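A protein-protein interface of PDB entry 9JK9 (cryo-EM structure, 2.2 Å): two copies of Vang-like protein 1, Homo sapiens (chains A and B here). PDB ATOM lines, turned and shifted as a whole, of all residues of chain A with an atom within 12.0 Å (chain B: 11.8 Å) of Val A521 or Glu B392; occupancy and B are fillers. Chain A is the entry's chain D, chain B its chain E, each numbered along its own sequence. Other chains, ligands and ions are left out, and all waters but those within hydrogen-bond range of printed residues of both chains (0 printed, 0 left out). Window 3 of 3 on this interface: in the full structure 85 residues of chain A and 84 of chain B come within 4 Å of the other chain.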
ATOM      1  N   LYS A 516       5.708 -11.124  27.880  1.00  0.00           N
ATOM      2  CA  LYS A 516       5.285 -11.629  26.583  1.00  0.00           C
ATOM      3  C   LYS A 516       6.340 -12.519  25.941  1.00  0.00           C
ATOM      4  O   LYS A 516       6.021 -13.251  25.001  1.00  0.00           O
ATOM      5  CB  LYS A 516       4.960 -10.462  25.652  1.00  0.00           C
ATOM      6  CG  LYS A 516       3.767  -9.632  26.089  1.00  0.00           C
ATOM      7  CD  LYS A 516       3.516  -8.490  25.119  1.00  0.00           C
ATOM      8  CE  LYS A 516       2.346  -7.633  25.567  1.00  0.00           C
ATOM      9  NZ  LYS A 516       2.106  -6.494  24.638  1.00  0.00           N
ATOM     10  N   SER A 517       7.583 -12.473  26.421  1.00  0.00           N
ATOM     11  CA  SER A 517       8.673 -13.254  25.848  1.00  0.00           C
ATOM     12  C   SER A 517       8.782 -14.653  26.439  1.00  0.00           C
ATOM     13  O   SER A 517       9.824 -15.297  26.280  1.00  0.00           O
ATOM     14  CB  SER A 517      10.003 -12.519  26.028  1.00  0.00           C
ATOM     15  OG  SER A 517      10.356 -12.439  27.397  1.00  0.00           O
ATOM     16  N   HIS A 518       7.736 -15.135  27.107  1.00  0.00           N
ATOM     17  CA  HIS A 518       7.684 -16.487  27.657  1.00  0.00           C
ATOM     18  C   HIS A 518       6.911 -17.423  26.745  1.00  0.00           C
ATOM     19  O   HIS A 518       6.102 -18.223  27.203  1.00  0.00           O
ATOM     20  CB  HIS A 518       7.084 -16.482  29.058  1.00  0.00           C
ATOM     21  CG  HIS A 518       7.933 -15.784  30.071  1.00  0.00           C
ATOM     22  ND1 HIS A 518       9.129 -16.299  30.518  1.00  0.00           N
ATOM     23  CD2 HIS A 518       7.750 -14.622  30.738  1.00  0.00           C
ATOM     24  CE1 HIS A 518       9.655 -15.475  31.407  1.00  0.00           C
ATOM     25  NE2 HIS A 518       8.837 -14.451  31.560  1.00  0.00           N
ATOM     26  N   LYS A 519       7.095 -17.286  25.440  1.00  0.00           N
ATOM     27  CA  LYS A 519       6.391 -18.119  24.484  1.00  0.00           C
ATOM     28  C   LYS A 519       7.159 -19.409  24.226  1.00  0.00           C
ATOM     29  O   LYS A 519       8.379 -19.406  24.067  1.00  0.00           O
ATOM     30  CB  LYS A 519       6.193 -17.352  23.181  1.00  0.00           C
ATOM     31  CG  LYS A 519       5.426 -16.057  23.355  1.00  0.00           C
ATOM     32  CD  LYS A 519       3.990 -16.311  23.768  1.00  0.00           C
ATOM     33  CE  LYS A 519       3.242 -15.006  23.980  1.00  0.00           C
ATOM     34  NZ  LYS A 519       3.053 -14.253  22.710  1.00  0.00           N
ATOM     35  N   PHE A 520       6.430 -20.519  24.180  1.00  0.00           N
ATOM     36  CA  PHE A 520       7.039 -21.834  24.046  1.00  0.00           C
ATOM     37  C   PHE A 520       6.456 -22.542  22.836  1.00  0.00           C
ATOM     38  O   PHE A 520       5.336 -22.256  22.410  1.00  0.00           O
ATOM     39  CB  PHE A 520       6.838 -22.667  25.322  1.00  0.00           C
ATOM     40  CG  PHE A 520       7.630 -22.158  26.482  1.00  0.00           C
ATOM     41  CD1 PHE A 520       8.925 -22.583  26.690  1.00  0.00           C
ATOM     42  CD2 PHE A 520       7.105 -21.196  27.320  1.00  0.00           C
ATOM     43  CE1 PHE A 520       9.667 -22.093  27.738  1.00  0.00           C
ATOM     44  CE2 PHE A 520       7.846 -20.689  28.361  1.00  0.00           C
ATOM     45  CZ  PHE A 520       9.130 -21.130  28.564  1.00  0.00           C
ATOM     46  N   VAL A 521       7.244 -23.447  22.265  1.00  0.00           N
ATOM     47  CA  VAL A 521       6.810 -24.240  21.127  1.00  0.00           C
ATOM     48  C   VAL A 521       6.865 -25.711  21.510  1.00  0.00           C
ATOM     49  O   VAL A 521       7.613 -26.126  22.396  1.00  0.00           O
ATOM     50  CB  VAL A 521       7.648 -23.971  19.859  1.00  0.00           C
ATOM     51  CG1 VAL A 521       7.447 -22.545  19.386  1.00  0.00           C
ATOM     52  CG2 VAL A 521       9.117 -24.236  20.119  1.00  0.00           C
ATOM     53  N   LEU A 522       6.047 -26.506  20.818  1.00  0.00           N
ATOM     54  CA  LEU A 522       6.011 -27.949  21.011  1.00  0.00           C
ATOM     55  C   LEU A 522       7.221 -28.644  20.395  1.00  0.00           C
ATOM     56  O   LEU A 522       7.414 -29.844  20.621  1.00  0.00           O
ATOM     57  CB  LEU A 522       4.700 -28.497  20.425  1.00  0.00           C
ATOM     58  CG  LEU A 522       4.204 -29.929  20.659  1.00  0.00           C
ATOM     59  CD1 LEU A 522       3.942 -30.166  22.136  1.00  0.00           C
ATOM     60  CD2 LEU A 522       2.960 -30.211  19.835  1.00  0.00           C
ATOM     61  N   ARG A 523       8.040 -27.914  19.640  1.00  0.00           N
ATOM     62  CA  ARG A 523       9.261 -28.454  19.065  1.00  0.00           C
ATOM     63  C   ARG A 523      10.242 -28.871  20.154  1.00  0.00           C
ATOM     64  O   ARG A 523      10.301 -28.281  21.235  1.00  0.00           O
ATOM     65  CB  ARG A 523       9.923 -27.423  18.151  1.00  0.00           C
ATOM     66  CG  ARG A 523       9.134 -27.092  16.897  1.00  0.00           C
ATOM     67  CD  ARG A 523       9.850 -26.031  16.075  1.00  0.00           C
ATOM     68  NE  ARG A 523      11.155 -26.497  15.611  1.00  0.00           N
ATOM     69  CZ  ARG A 523      11.352 -27.175  14.485  1.00  0.00           C
ATOM     70  NH1 ARG A 523      10.327 -27.471  13.698  1.00  0.00           N
ATOM     71  NH2 ARG A 523      12.575 -27.558  14.145  1.00  0.00           N
ATOM     72  N   LEU A 524      11.006 -29.912  19.855  1.00  0.00           N
ATOM     73  CA  LEU A 524      11.980 -30.438  20.794  1.00  0.00           C
ATOM     74  C   LEU A 524      13.169 -29.486  20.905  1.00  0.00           C
ATOM     75  O   LEU A 524      13.495 -28.761  19.962  1.00  0.00           O
ATOM     76  CB  LEU A 524      12.442 -31.813  20.320  1.00  0.00           C
ATOM     77  CG  LEU A 524      11.359 -32.871  20.074  1.00  0.00           C
ATOM     78  CD1 LEU A 524      11.961 -34.141  19.476  1.00  0.00           C
ATOM     79  CD2 LEU A 524      10.558 -33.187  21.326  1.00  0.00           C
ATOM     80  N   GLN A 525      13.816 -29.481  22.068  1.00  0.00           N
ATOM     81  CA  GLN A 525      14.994 -28.627  22.237  1.00  0.00           C
ATOM     82  C   GLN A 525      16.272 -29.448  22.363  1.00  0.00           C
ATOM     83  O   GLN A 525      16.246 -30.601  22.788  1.00  0.00           O
ATOM     84  CB  GLN A 525      14.855 -27.706  23.454  1.00  0.00           C
ATOM     85  CG  GLN A 525      14.902 -28.395  24.799  1.00  0.00           C
ATOM     86  CD  GLN A 525      14.786 -27.425  25.959  1.00  0.00           C
ATOM     87  OE1 GLN A 525      14.728 -26.211  25.763  1.00  0.00           O
ATOM     88  NE2 GLN A 525      14.749 -27.957  27.174  1.00  0.00           N
ATOM     89  N   GLU B 373      12.366 -35.948  30.567  1.00  0.00           N
ATOM     90  CA  GLU B 373      11.889 -36.148  29.209  1.00  0.00           C
ATOM     91  C   GLU B 373      10.573 -35.425  28.948  1.00  0.00           C
ATOM     92  O   GLU B 373      10.148 -35.335  27.795  1.00  0.00           O
ATOM     93  CB  GLU B 373      11.764 -37.639  28.912  1.00  0.00           C
ATOM     94  CG  GLU B 373      13.095 -38.368  29.027  1.00  0.00           C
ATOM     95  CD  GLU B 373      13.030 -39.796  28.537  1.00  0.00           C
ATOM     96  OE1 GLU B 373      11.948 -40.221  28.084  1.00  0.00           O
ATOM     97  OE2 GLU B 373      14.059 -40.498  28.612  1.00  0.00           O
ATOM     98  N   ALA B 374       9.925 -34.904  29.988  1.00  0.00           N
ATOM     99  CA  ALA B 374       8.798 -34.006  29.778  1.00  0.00           C
ATOM    100  C   ALA B 374       9.266 -32.586  29.484  1.00  0.00           C
ATOM    101  O   ALA B 374       8.717 -31.925  28.595  1.00  0.00           O
ATOM    102  CB  ALA B 374       7.887 -34.031  30.996  1.00  0.00           C
ATOM    103  N   PHE B 375      10.276 -32.094  30.214  1.00  0.00           N
ATOM    104  CA  PHE B 375      10.745 -30.731  29.963  1.00  0.00           C
ATOM    105  C   PHE B 375      11.502 -30.610  28.660  1.00  0.00           C
ATOM    106  O   PHE B 375      11.628 -29.499  28.134  1.00  0.00           O
ATOM    107  CB  PHE B 375      11.674 -30.174  31.050  1.00  0.00           C
ATOM    108  CG  PHE B 375      10.989 -29.752  32.315  1.00  0.00           C
ATOM    109  CD1 PHE B 375       9.691 -30.109  32.591  1.00  0.00           C
ATOM    110  CD2 PHE B 375      11.611 -28.853  33.156  1.00  0.00           C
ATOM    111  CE1 PHE B 375       9.089 -29.698  33.733  1.00  0.00           C
ATOM    112  CE2 PHE B 375      10.996 -28.418  34.298  1.00  0.00           C
ATOM    113  CZ  PHE B 375       9.728 -28.838  34.580  1.00  0.00           C
ATOM    114  N   ILE B 376      12.011 -31.719  28.125  1.00  0.00           N
ATOM    115  CA  ILE B 376      12.716 -31.631  26.856  1.00  0.00           C
ATOM    116  C   ILE B 376      11.750 -31.493  25.670  1.00  0.00           C
ATOM    117  O   ILE B 376      12.190 -31.249  24.541  1.00  0.00           O
ATOM    118  CB  ILE B 376      13.645 -32.853  26.749  1.00  0.00           C
ATOM    119  CG1 ILE B 376      14.819 -32.571  25.818  1.00  0.00           C
ATOM    120  CG2 ILE B 376      12.869 -34.053  26.289  1.00  0.00           C
ATOM    121  CD1 ILE B 376      15.725 -31.483  26.313  1.00  0.00           C
ATOM    122  N   HIS B 377      10.435 -31.587  25.899  1.00  0.00           N
ATOM    123  CA  HIS B 377       9.484 -31.570  24.790  1.00  0.00           C
ATOM    124  C   HIS B 377       9.127 -30.156  24.342  1.00  0.00           C
ATOM    125  O   HIS B 377       8.530 -29.979  23.275  1.00  0.00           O
ATOM    126  CB  HIS B 377       8.215 -32.329  25.169  1.00  0.00           C
ATOM    127  CG  HIS B 377       8.385 -33.813  25.204  1.00  0.00           C
ATOM    128  ND1 HIS B 377       7.425 -34.660  25.716  1.00  0.00           N
ATOM    129  CD2 HIS B 377       9.396 -34.605  24.778  1.00  0.00           C
ATOM    130  CE1 HIS B 377       7.842 -35.909  25.611  1.00  0.00           C
ATOM    131  NE2 HIS B 377       9.036 -35.903  25.047  1.00  0.00           N
ATOM    132  N   ILE B 378       9.452 -29.144  25.132  1.00  0.00           N
ATOM    133  CA  ILE B 378       9.149 -27.765  24.759  1.00  0.00           C
ATOM    134  C   ILE B 378      10.423 -26.941  24.737  1.00  0.00           C
ATOM    135  O   ILE B 378      11.429 -27.290  25.359  1.00  0.00           O
ATOM    136  CB  ILE B 378       8.101 -27.125  25.692  1.00  0.00           C
ATOM    137  CG1 ILE B 378       8.527 -27.264  27.154  1.00  0.00           C
ATOM    138  CG2 ILE B 378       6.716 -27.678  25.403  1.00  0.00           C
ATOM    139  CD1 ILE B 378       7.690 -26.459  28.104  1.00  0.00           C
ATOM    140  N   GLN B 379      10.370 -25.821  24.024  1.00  0.00           N
ATOM    141  CA  GLN B 379      11.527 -24.982  23.755  1.00  0.00           C
ATOM    142  C   GLN B 379      11.197 -23.530  24.086  1.00  0.00           C
ATOM    143  O   GLN B 379      10.068 -23.076  23.885  1.00  0.00           O
ATOM    144  CB  GLN B 379      11.950 -25.125  22.288  1.00  0.00           C
ATOM    145  CG  GLN B 379      13.249 -24.453  21.896  1.00  0.00           C
ATOM    146  CD  GLN B 379      13.625 -24.738  20.461  1.00  0.00           C
ATOM    147  OE1 GLN B 379      12.893 -25.417  19.742  1.00  0.00           O
ATOM    148  NE2 GLN B 379      14.772 -24.225  20.035  1.00  0.00           N
ATOM    149  N   ARG B 380      12.209 -22.801  24.573  1.00  0.00           N
ATOM    150  CA  ARG B 380      12.005 -21.463  25.129  1.00  0.00           C
ATOM    151  C   ARG B 380      11.652 -20.444  24.047  1.00  0.00           C
ATOM    152  O   ARG B 380      11.059 -19.399  24.346  1.00  0.00           O
ATOM    153  CB  ARG B 380      13.264 -21.051  25.908  1.00  0.00           C
ATOM    154  CG  ARG B 380      13.256 -19.682  26.598  1.00  0.00           C
ATOM    155  CD  ARG B 380      12.164 -19.610  27.640  1.00  0.00           C
ATOM    156  NE  ARG B 380      12.106 -18.325  28.326  1.00  0.00           N
ATOM    157  CZ  ARG B 380      12.738 -18.058  29.463  1.00  0.00           C
ATOM    158  NH1 ARG B 380      13.479 -18.991  30.047  1.00  0.00           N
ATOM    159  NH2 ARG B 380      12.629 -16.859  30.019  1.00  0.00           N
ATOM    160  N   LEU B 381      11.981 -20.747  22.787  1.00  0.00           N
ATOM    161  CA  LEU B 381      11.687 -19.914  21.605  1.00  0.00           C
ATOM    162  C   LEU B 381      12.255 -18.497  21.700  1.00  0.00           C
ATOM    163  O   LEU B 381      13.008 -18.062  20.829  1.00  0.00           O
ATOM    164  CB  LEU B 381      10.173 -19.845  21.342  1.00  0.00           C
ATOM    165  CG  LEU B 381       9.720 -18.999  20.153  1.00  0.00           C
ATOM    166  CD1 LEU B 381      10.202 -19.604  18.845  1.00  0.00           C
ATOM    167  CD2 LEU B 381       8.208 -18.822  20.156  1.00  0.00           C
ATOM    168  N   GLU B 392       3.606 -24.254  16.939  1.00  0.00           N
ATOM    169  CA  GLU B 392       2.530 -23.467  17.529  1.00  0.00           C
ATOM    170  C   GLU B 392       2.965 -22.795  18.827  1.00  0.00           C
ATOM    171  O   GLU B 392       3.522 -23.431  19.717  1.00  0.00           O
ATOM    172  CB  GLU B 392       1.297 -24.341  17.777  1.00  0.00           C
ATOM    173  CG  GLU B 392       0.122 -23.605  18.408  1.00  0.00           C
ATOM    174  CD  GLU B 392      -0.472 -22.532  17.509  1.00  0.00           C
ATOM    175  OE1 GLU B 392      -0.401 -22.670  16.269  1.00  0.00           O
ATOM    176  OE2 GLU B 392      -1.011 -21.543  18.048  1.00  0.00           O
ATOM    177  N   VAL B 393       2.691 -21.492  18.915  1.00  0.00           N
ATOM    178  CA  VAL B 393       3.117 -20.699  20.058  1.00  0.00           C
ATOM    179  C   VAL B 393       2.091 -20.803  21.181  1.00  0.00           C
ATOM    180  O   VAL B 393       0.880 -20.693  20.955  1.00  0.00           O
ATOM    181  CB  VAL B 393       3.327 -19.247  19.597  1.00  0.00           C
ATOM    182  CG1 VAL B 393       3.574 -18.328  20.755  1.00  0.00           C
ATOM    183  CG2 VAL B 393       4.487 -19.179  18.615  1.00  0.00           C
ATOM    184  N   MET B 394       2.574 -21.027  22.405  1.00  0.00           N
ATOM    185  CA  MET B 394       1.704 -21.136  23.568  1.00  0.00           C
ATOM    186  C   MET B 394       2.381 -20.541  24.798  1.00  0.00           C
ATOM    187  O   MET B 394       3.606 -20.472  24.891  1.00  0.00           O
ATOM    188  CB  MET B 394       1.291 -22.597  23.807  1.00  0.00           C
ATOM    189  CG  MET B 394       2.443 -23.570  23.957  1.00  0.00           C
ATOM    190  SD  MET B 394       1.888 -25.283  24.013  1.00  0.00           S
ATOM    191  CE  MET B 394       3.450 -26.148  23.972  1.00  0.00           C
ATOM    192  N   ASP B 395       1.546 -20.092  25.737  1.00  0.00           N
ATOM    193  CA  ASP B 395       1.960 -19.518  27.011  1.00  0.00           C
ATOM    194  C   ASP B 395       2.393 -20.646  27.963  1.00  0.00           C
ATOM    195  O   ASP B 395       2.187 -21.820  27.645  1.00  0.00           O
ATOM    196  CB  ASP B 395       0.809 -18.658  27.556  1.00  0.00           C
ATOM    197  CG  ASP B 395      -0.488 -19.417  27.707  1.00  0.00           C
ATOM    198  OD1 ASP B 395      -0.569 -20.568  27.254  1.00  0.00           O
ATOM    199  OD2 ASP B 395      -1.435 -18.854  28.294  1.00  0.00           O
ATOM    200  N   PRO B 396       3.038 -20.338  29.109  1.00  0.00           N
ATOM    201  CA  PRO B 396       3.513 -21.432  29.982  1.00  0.00           C
ATOM    202  C   PRO B 396       2.424 -22.303  30.585  1.00  0.00           C
ATOM    203  O   PRO B 396       2.718 -23.445  30.953  1.00  0.00           O
ATOM    204  CB  PRO B 396       4.287 -20.697  31.081  1.00  0.00           C
ATOM    205  CG  PRO B 396       4.713 -19.463  30.468  1.00  0.00           C
ATOM    206  CD  PRO B 396       3.615 -19.055  29.567  1.00  0.00           C
ATOM    207  N   ARG B 397       1.188 -21.816  30.688  1.00  0.00           N
ATOM    208  CA  ARG B 397       0.097 -22.658  31.165  1.00  0.00           C
ATOM    209  C   ARG B 397      -0.221 -23.764  30.164  1.00  0.00           C
ATOM    210  O   ARG B 397      -0.348 -24.937  30.534  1.00  0.00           O
ATOM    211  CB  ARG B 397      -1.140 -21.803  31.428  1.00  0.00           C
ATOM    212  CG  ARG B 397      -2.328 -22.592  31.922  1.00  0.00           C
ATOM    213  CD  ARG B 397      -2.128 -23.059  33.347  1.00  0.00           C
ATOM    214  NE  ARG B 397      -3.254 -23.866  33.798  1.00  0.00           N
ATOM    215  CZ  ARG B 397      -3.329 -24.441  34.991  1.00  0.00           C
ATOM    216  NH1 ARG B 397      -2.350 -24.275  35.870  1.00  0.00           N
ATOM    217  NH2 ARG B 397      -4.388 -25.166  35.311  1.00  0.00           N
ATOM    218  N   GLU B 398      -0.318 -23.412  28.879  1.00  0.00           N
ATOM    219  CA  GLU B 398      -0.591 -24.413  27.853  1.00  0.00           C
ATOM    220  C   GLU B 398       0.617 -25.303  27.592  1.00  0.00           C
ATOM    221  O   GLU B 398       0.447 -26.476  27.251  1.00  0.00           O
ATOM    222  CB  GLU B 398      -1.051 -23.732  26.567  1.00  0.00           C
ATOM    223  CG  GLU B 398      -2.452 -23.145  26.659  1.00  0.00           C
ATOM    224  CD  GLU B 398      -2.816 -22.306  25.447  1.00  0.00           C
ATOM    225  OE1 GLU B 398      -1.931 -22.058  24.604  1.00  0.00           O
ATOM    226  OE2 GLU B 398      -3.987 -21.885  25.339  1.00  0.00           O
ATOM    227  N   ALA B 399       1.834 -24.786  27.776  1.00  0.00           N
ATOM    228  CA  ALA B 399       3.018 -25.637  27.679  1.00  0.00           C
ATOM    229  C   ALA B 399       3.080 -26.632  28.833  1.00  0.00           C
ATOM    230  O   ALA B 399       3.473 -27.794  28.645  1.00  0.00           O
ATOM    231  CB  ALA B 399       4.279 -24.776  27.646  1.00  0.00           C
ATOM    232  N   ALA B 400       2.677 -26.192  30.029  1.00  0.00           N
ATOM    233  CA  ALA B 400       2.569 -27.080  31.180  1.00  0.00           C
ATOM    234  C   ALA B 400       1.526 -28.163  30.942  1.00  0.00           C
ATOM    235  O   ALA B 400       1.760 -29.342  31.230  1.00  0.00           O
ATOM    236  CB  ALA B 400       2.218 -26.264  32.422  1.00  0.00           C
ATOM    237  N   GLN B 401       0.370 -27.778  30.396  1.00  0.00           N
ATOM    238  CA  GLN B 401      -0.672 -28.750  30.075  1.00  0.00           C
ATOM    239  C   GLN B 401      -0.254 -29.679  28.942  1.00  0.00           C
ATOM    240  O   GLN B 401      -0.741 -30.810  28.861  1.00  0.00           O
ATOM    241  CB  GLN B 401      -1.966 -28.029  29.712  1.00  0.00           C
ATOM    242  CG  GLN B 401      -2.619 -27.317  30.876  1.00  0.00           C
ATOM    243  CD  GLN B 401      -3.841 -26.533  30.461  1.00  0.00           C
ATOM    244  OE1 GLN B 401      -4.166 -26.454  29.277  1.00  0.00           O
ATOM    245  NE2 GLN B 401      -4.526 -25.945  31.433  1.00  0.00           N
ATOM    246  N   ALA B 402       0.633 -29.218  28.060  1.00  0.00           N
ATOM    247  CA  ALA B 402       1.130 -30.067  26.987  1.00  0.00           C
ATOM    248  C   ALA B 402       2.074 -31.135  27.519  1.00  0.00           C
ATOM    249  O   ALA B 402       1.940 -32.316  27.184  1.00  0.00           O
ATOM    250  CB  ALA B 402       1.827 -29.215  25.927  1.00  0.00           C
ATOM    251  N   ILE B 403       3.038 -30.742  28.358  1.00  0.00           N
ATOM    252  CA  ILE B 403       4.053 -31.703  28.791  1.00  0.00           C
ATOM    253  C   ILE B 403       3.681 -32.471  30.050  1.00  0.00           C
ATOM    254  O   ILE B 403       4.389 -33.425  30.403  1.00  0.00           O
ATOM    255  CB  ILE B 403       5.420 -31.042  29.035  1.00  0.00           C
ATOM    256  CG1 ILE B 403       5.344 -30.057  30.196  1.00  0.00           C
ATOM    257  CG2 ILE B 403       5.897 -30.368  27.779  1.00  0.00           C
ATOM    258  CD1 ILE B 403       6.688 -29.596  30.652  1.00  0.00           C
ATOM    259  N   PHE B 404       2.609 -32.092  30.739  1.00  0.00           N
ATOM    260  CA  PHE B 404       2.212 -32.818  31.945  1.00  0.00           C
ATOM    261  C   PHE B 404       1.747 -34.268  31.752  1.00  0.00           C
ATOM    262  O   PHE B 404       2.054 -35.082  32.645  1.00  0.00           O
ATOM    263  CB  PHE B 404       1.145 -32.004  32.687  1.00  0.00           C
ATOM    264  CG  PHE B 404       0.657 -32.654  33.943  1.00  0.00           C
ATOM    265  CD1 PHE B 404       1.474 -32.734  35.057  1.00  0.00           C
ATOM    266  CD2 PHE B 404      -0.622 -33.181  34.014  1.00  0.00           C
ATOM    267  CE1 PHE B 404       1.030 -33.338  36.213  1.00  0.00           C
ATOM    268  CE2 PHE B 404      -1.074 -33.781  35.170  1.00  0.00           C
ATOM    269  CZ  PHE B 404      -0.245 -33.857  36.272  1.00  0.00           C
ATOM    270  N   ILE B 437       8.366 -23.523  34.267  1.00  0.00           N
ATOM    271  CA  ILE B 437       8.594 -23.296  32.842  1.00  0.00           C
ATOM    272  C   ILE B 437       8.807 -21.810  32.563  1.00  0.00           C
ATOM    273  O   ILE B 437       9.648 -21.437  31.736  1.00  0.00           O
ATOM    274  CB  ILE B 437       7.422 -23.896  32.037  1.00  0.00           C
ATOM    275  CG1 ILE B 437       7.470 -25.418  32.067  1.00  0.00           C
ATOM    276  CG2 ILE B 437       7.434 -23.494  30.601  1.00  0.00           C
ATOM    277  CD1 ILE B 437       6.204 -26.042  31.564  1.00  0.00           C
ATOM    278  N   THR B 438       8.081 -20.943  33.278  1.00  0.00           N
ATOM    279  CA  THR B 438       8.241 -19.496  33.131  1.00  0.00           C
ATOM    280  C   THR B 438       9.630 -19.037  33.556  1.00  0.00           C
ATOM    281  O   THR B 438      10.307 -18.302  32.829  1.00  0.00           O
ATOM    282  CB  THR B 438       7.180 -18.768  33.957  1.00  0.00           C
ATOM    283  OG1 THR B 438       5.875 -19.159  33.527  1.00  0.00           O
ATOM    284  CG2 THR B 438       7.321 -17.266  33.811  1.00  0.00           C
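ND1 of His A518 lies close to O of Thr B438 (3.3 Å).
The backbone carbonyl oxygen (O) of Lys A519 lies close to the backbone carbonyl oxygen (O) of Arg B380 (2.7 Å).
The backbone carbonyl oxygen of Met B394 sits at hydrogen-bond distance from the backbone NH of Phe A520.
The backbone NH (N) of Gln B379 sits at hydrogen-bond distance from the backbone carbonyl oxygen (O) of Val A521 (3.2 Å).
O of Leu A524 sits close to OE1 of Gln B379 (3.4 Å).
The backbone carbonyl oxygen (O) of Ile B376 lies within hydrogen-bond range of the backbone NH (N) of Gln A525 (3.4 Å).
O of Ile B378 sits close to OE1 of Gln A525, 3.5 Å away.
O of Glu B392 lies close to O of Phe A520 (3.5 Å).
O of His B377 sits close to O of Leu A522.
The backbone carbonyl oxygen (O) of Arg A523 lies close to the backbone carbonyl oxygen (O) of His B377, 3.2 Å away.
The backbone carbonyl oxygen (O) of Glu B373 sits at hydrogen-bond distance from a ring nitrogen (NE2) of His B377.
The side-chain sulfur (SD) of Met B394 is in hydrogen-bond range of the backbone NH (N) of Ala B399, 3.8 Å away.
Among the printed residues, pairs that only touch across the chains: Phe A520 with Gln B379, Phe A520 with Ile B437, Val A521 with Ile B378, Lys A519 with Leu B381, Phe A520 with Arg B380, His A518 with Pro B396, His A518 with Arg B380, Phe A520 with Val B393, Gln A525 with Phe B375, Lys A519 with Val B393, Val A521 with Glu B392, Lys A519 with Met B394, Arg A523 with Gln B379, Arg A523 with Ile B378, Leu A524 with Ile B376, Val A521 with Leu B381, Leu A524 with His B377, Gln A525 with Gln B379 and Phe A520 with Pro B396.
Of chain B, only Ile B378 (3.3 Å), Gln B379 (3.2 Å), Leu B381 (3.9 Å) and Glu B392 (3.7 Å) come within 4 Å of Val A521.
Of chain A, only Phe A520 and Val A521 come within 4 Å of Glu B392.
Phe A520 touches just these residues of chain B: Gln B379, Arg B380, Glu B392, Val B393, Met B394, Pro B396 and Ile B437.
Of chain B, only His B377, Ile B378 and Gln B379 come within 4 Å of Arg A523.
Of chain A, only Phe A520 (3.1 Å), Val A521 (3.2 Å), Arg A523 (3.7 Å), Leu A524 (3.4 Å) and Gln A525 (3.9 Å) come within 4 Å of Gln B379.
Leu B381 touches just these residues of chain A: Lys A519 and Val A521.
Of chain A, only Lys A519 and Phe A520 come within 4 Å of Val B393.
Of chain A, only Lys A519 and Phe A520 come within 4 Å of Met B394.
Ala B399 touches none of the printed residues of chain A.
Of the printed residues of chain A, Arg B380 touches His A518, Lys A519 and Phe A520.
Printed residues of chain A within 4 Å of Phe B375: Gln A525.
Of the printed residues of chain B, Gln A525 touches Phe B375, Ile B376, Ile B378 and Gln B379.
Ile B403 touches none of the printed residues of chain A.
Asp B395 touches none of the printed residues of chain A.
The nearest residue of chain B that does not touch Val A521 is His B377 (4.1 Å).
The nearest printed residue of chain A that does not touch Ile B376 is Arg A523 (4.8 Å).
Printed residues of chain B that touch a printed residue of chain A: Phe B375, Ile B376, His B377, Ile B378, Gln B379, Arg B380, Leu B381, Glu B392, Val B393, Met B394, Pro B396, Ile B437 and Thr B438.
Hydrophobic or aromatic side chains of chain B within 4 Å of the printed part of chain A: Ile B376, His B377, Ile B378, Leu B381, Val B393, Met B394, Pro B396 and Ile B437.
Hydrophobic or aromatic side chains of chain A that line the printed part of chain B: His A518, Phe A520, Val A521 and Leu A524.
Along chain A the printed residues that touch a printed residue of chain B span positions 518 to 525.
Among the printed residues, 29 pairs touch across the chains.
No position is printed for both chains.
Of the 29 pairs that touch across the chains among the printed residues, none has its exchanged pair printed and touching as well.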
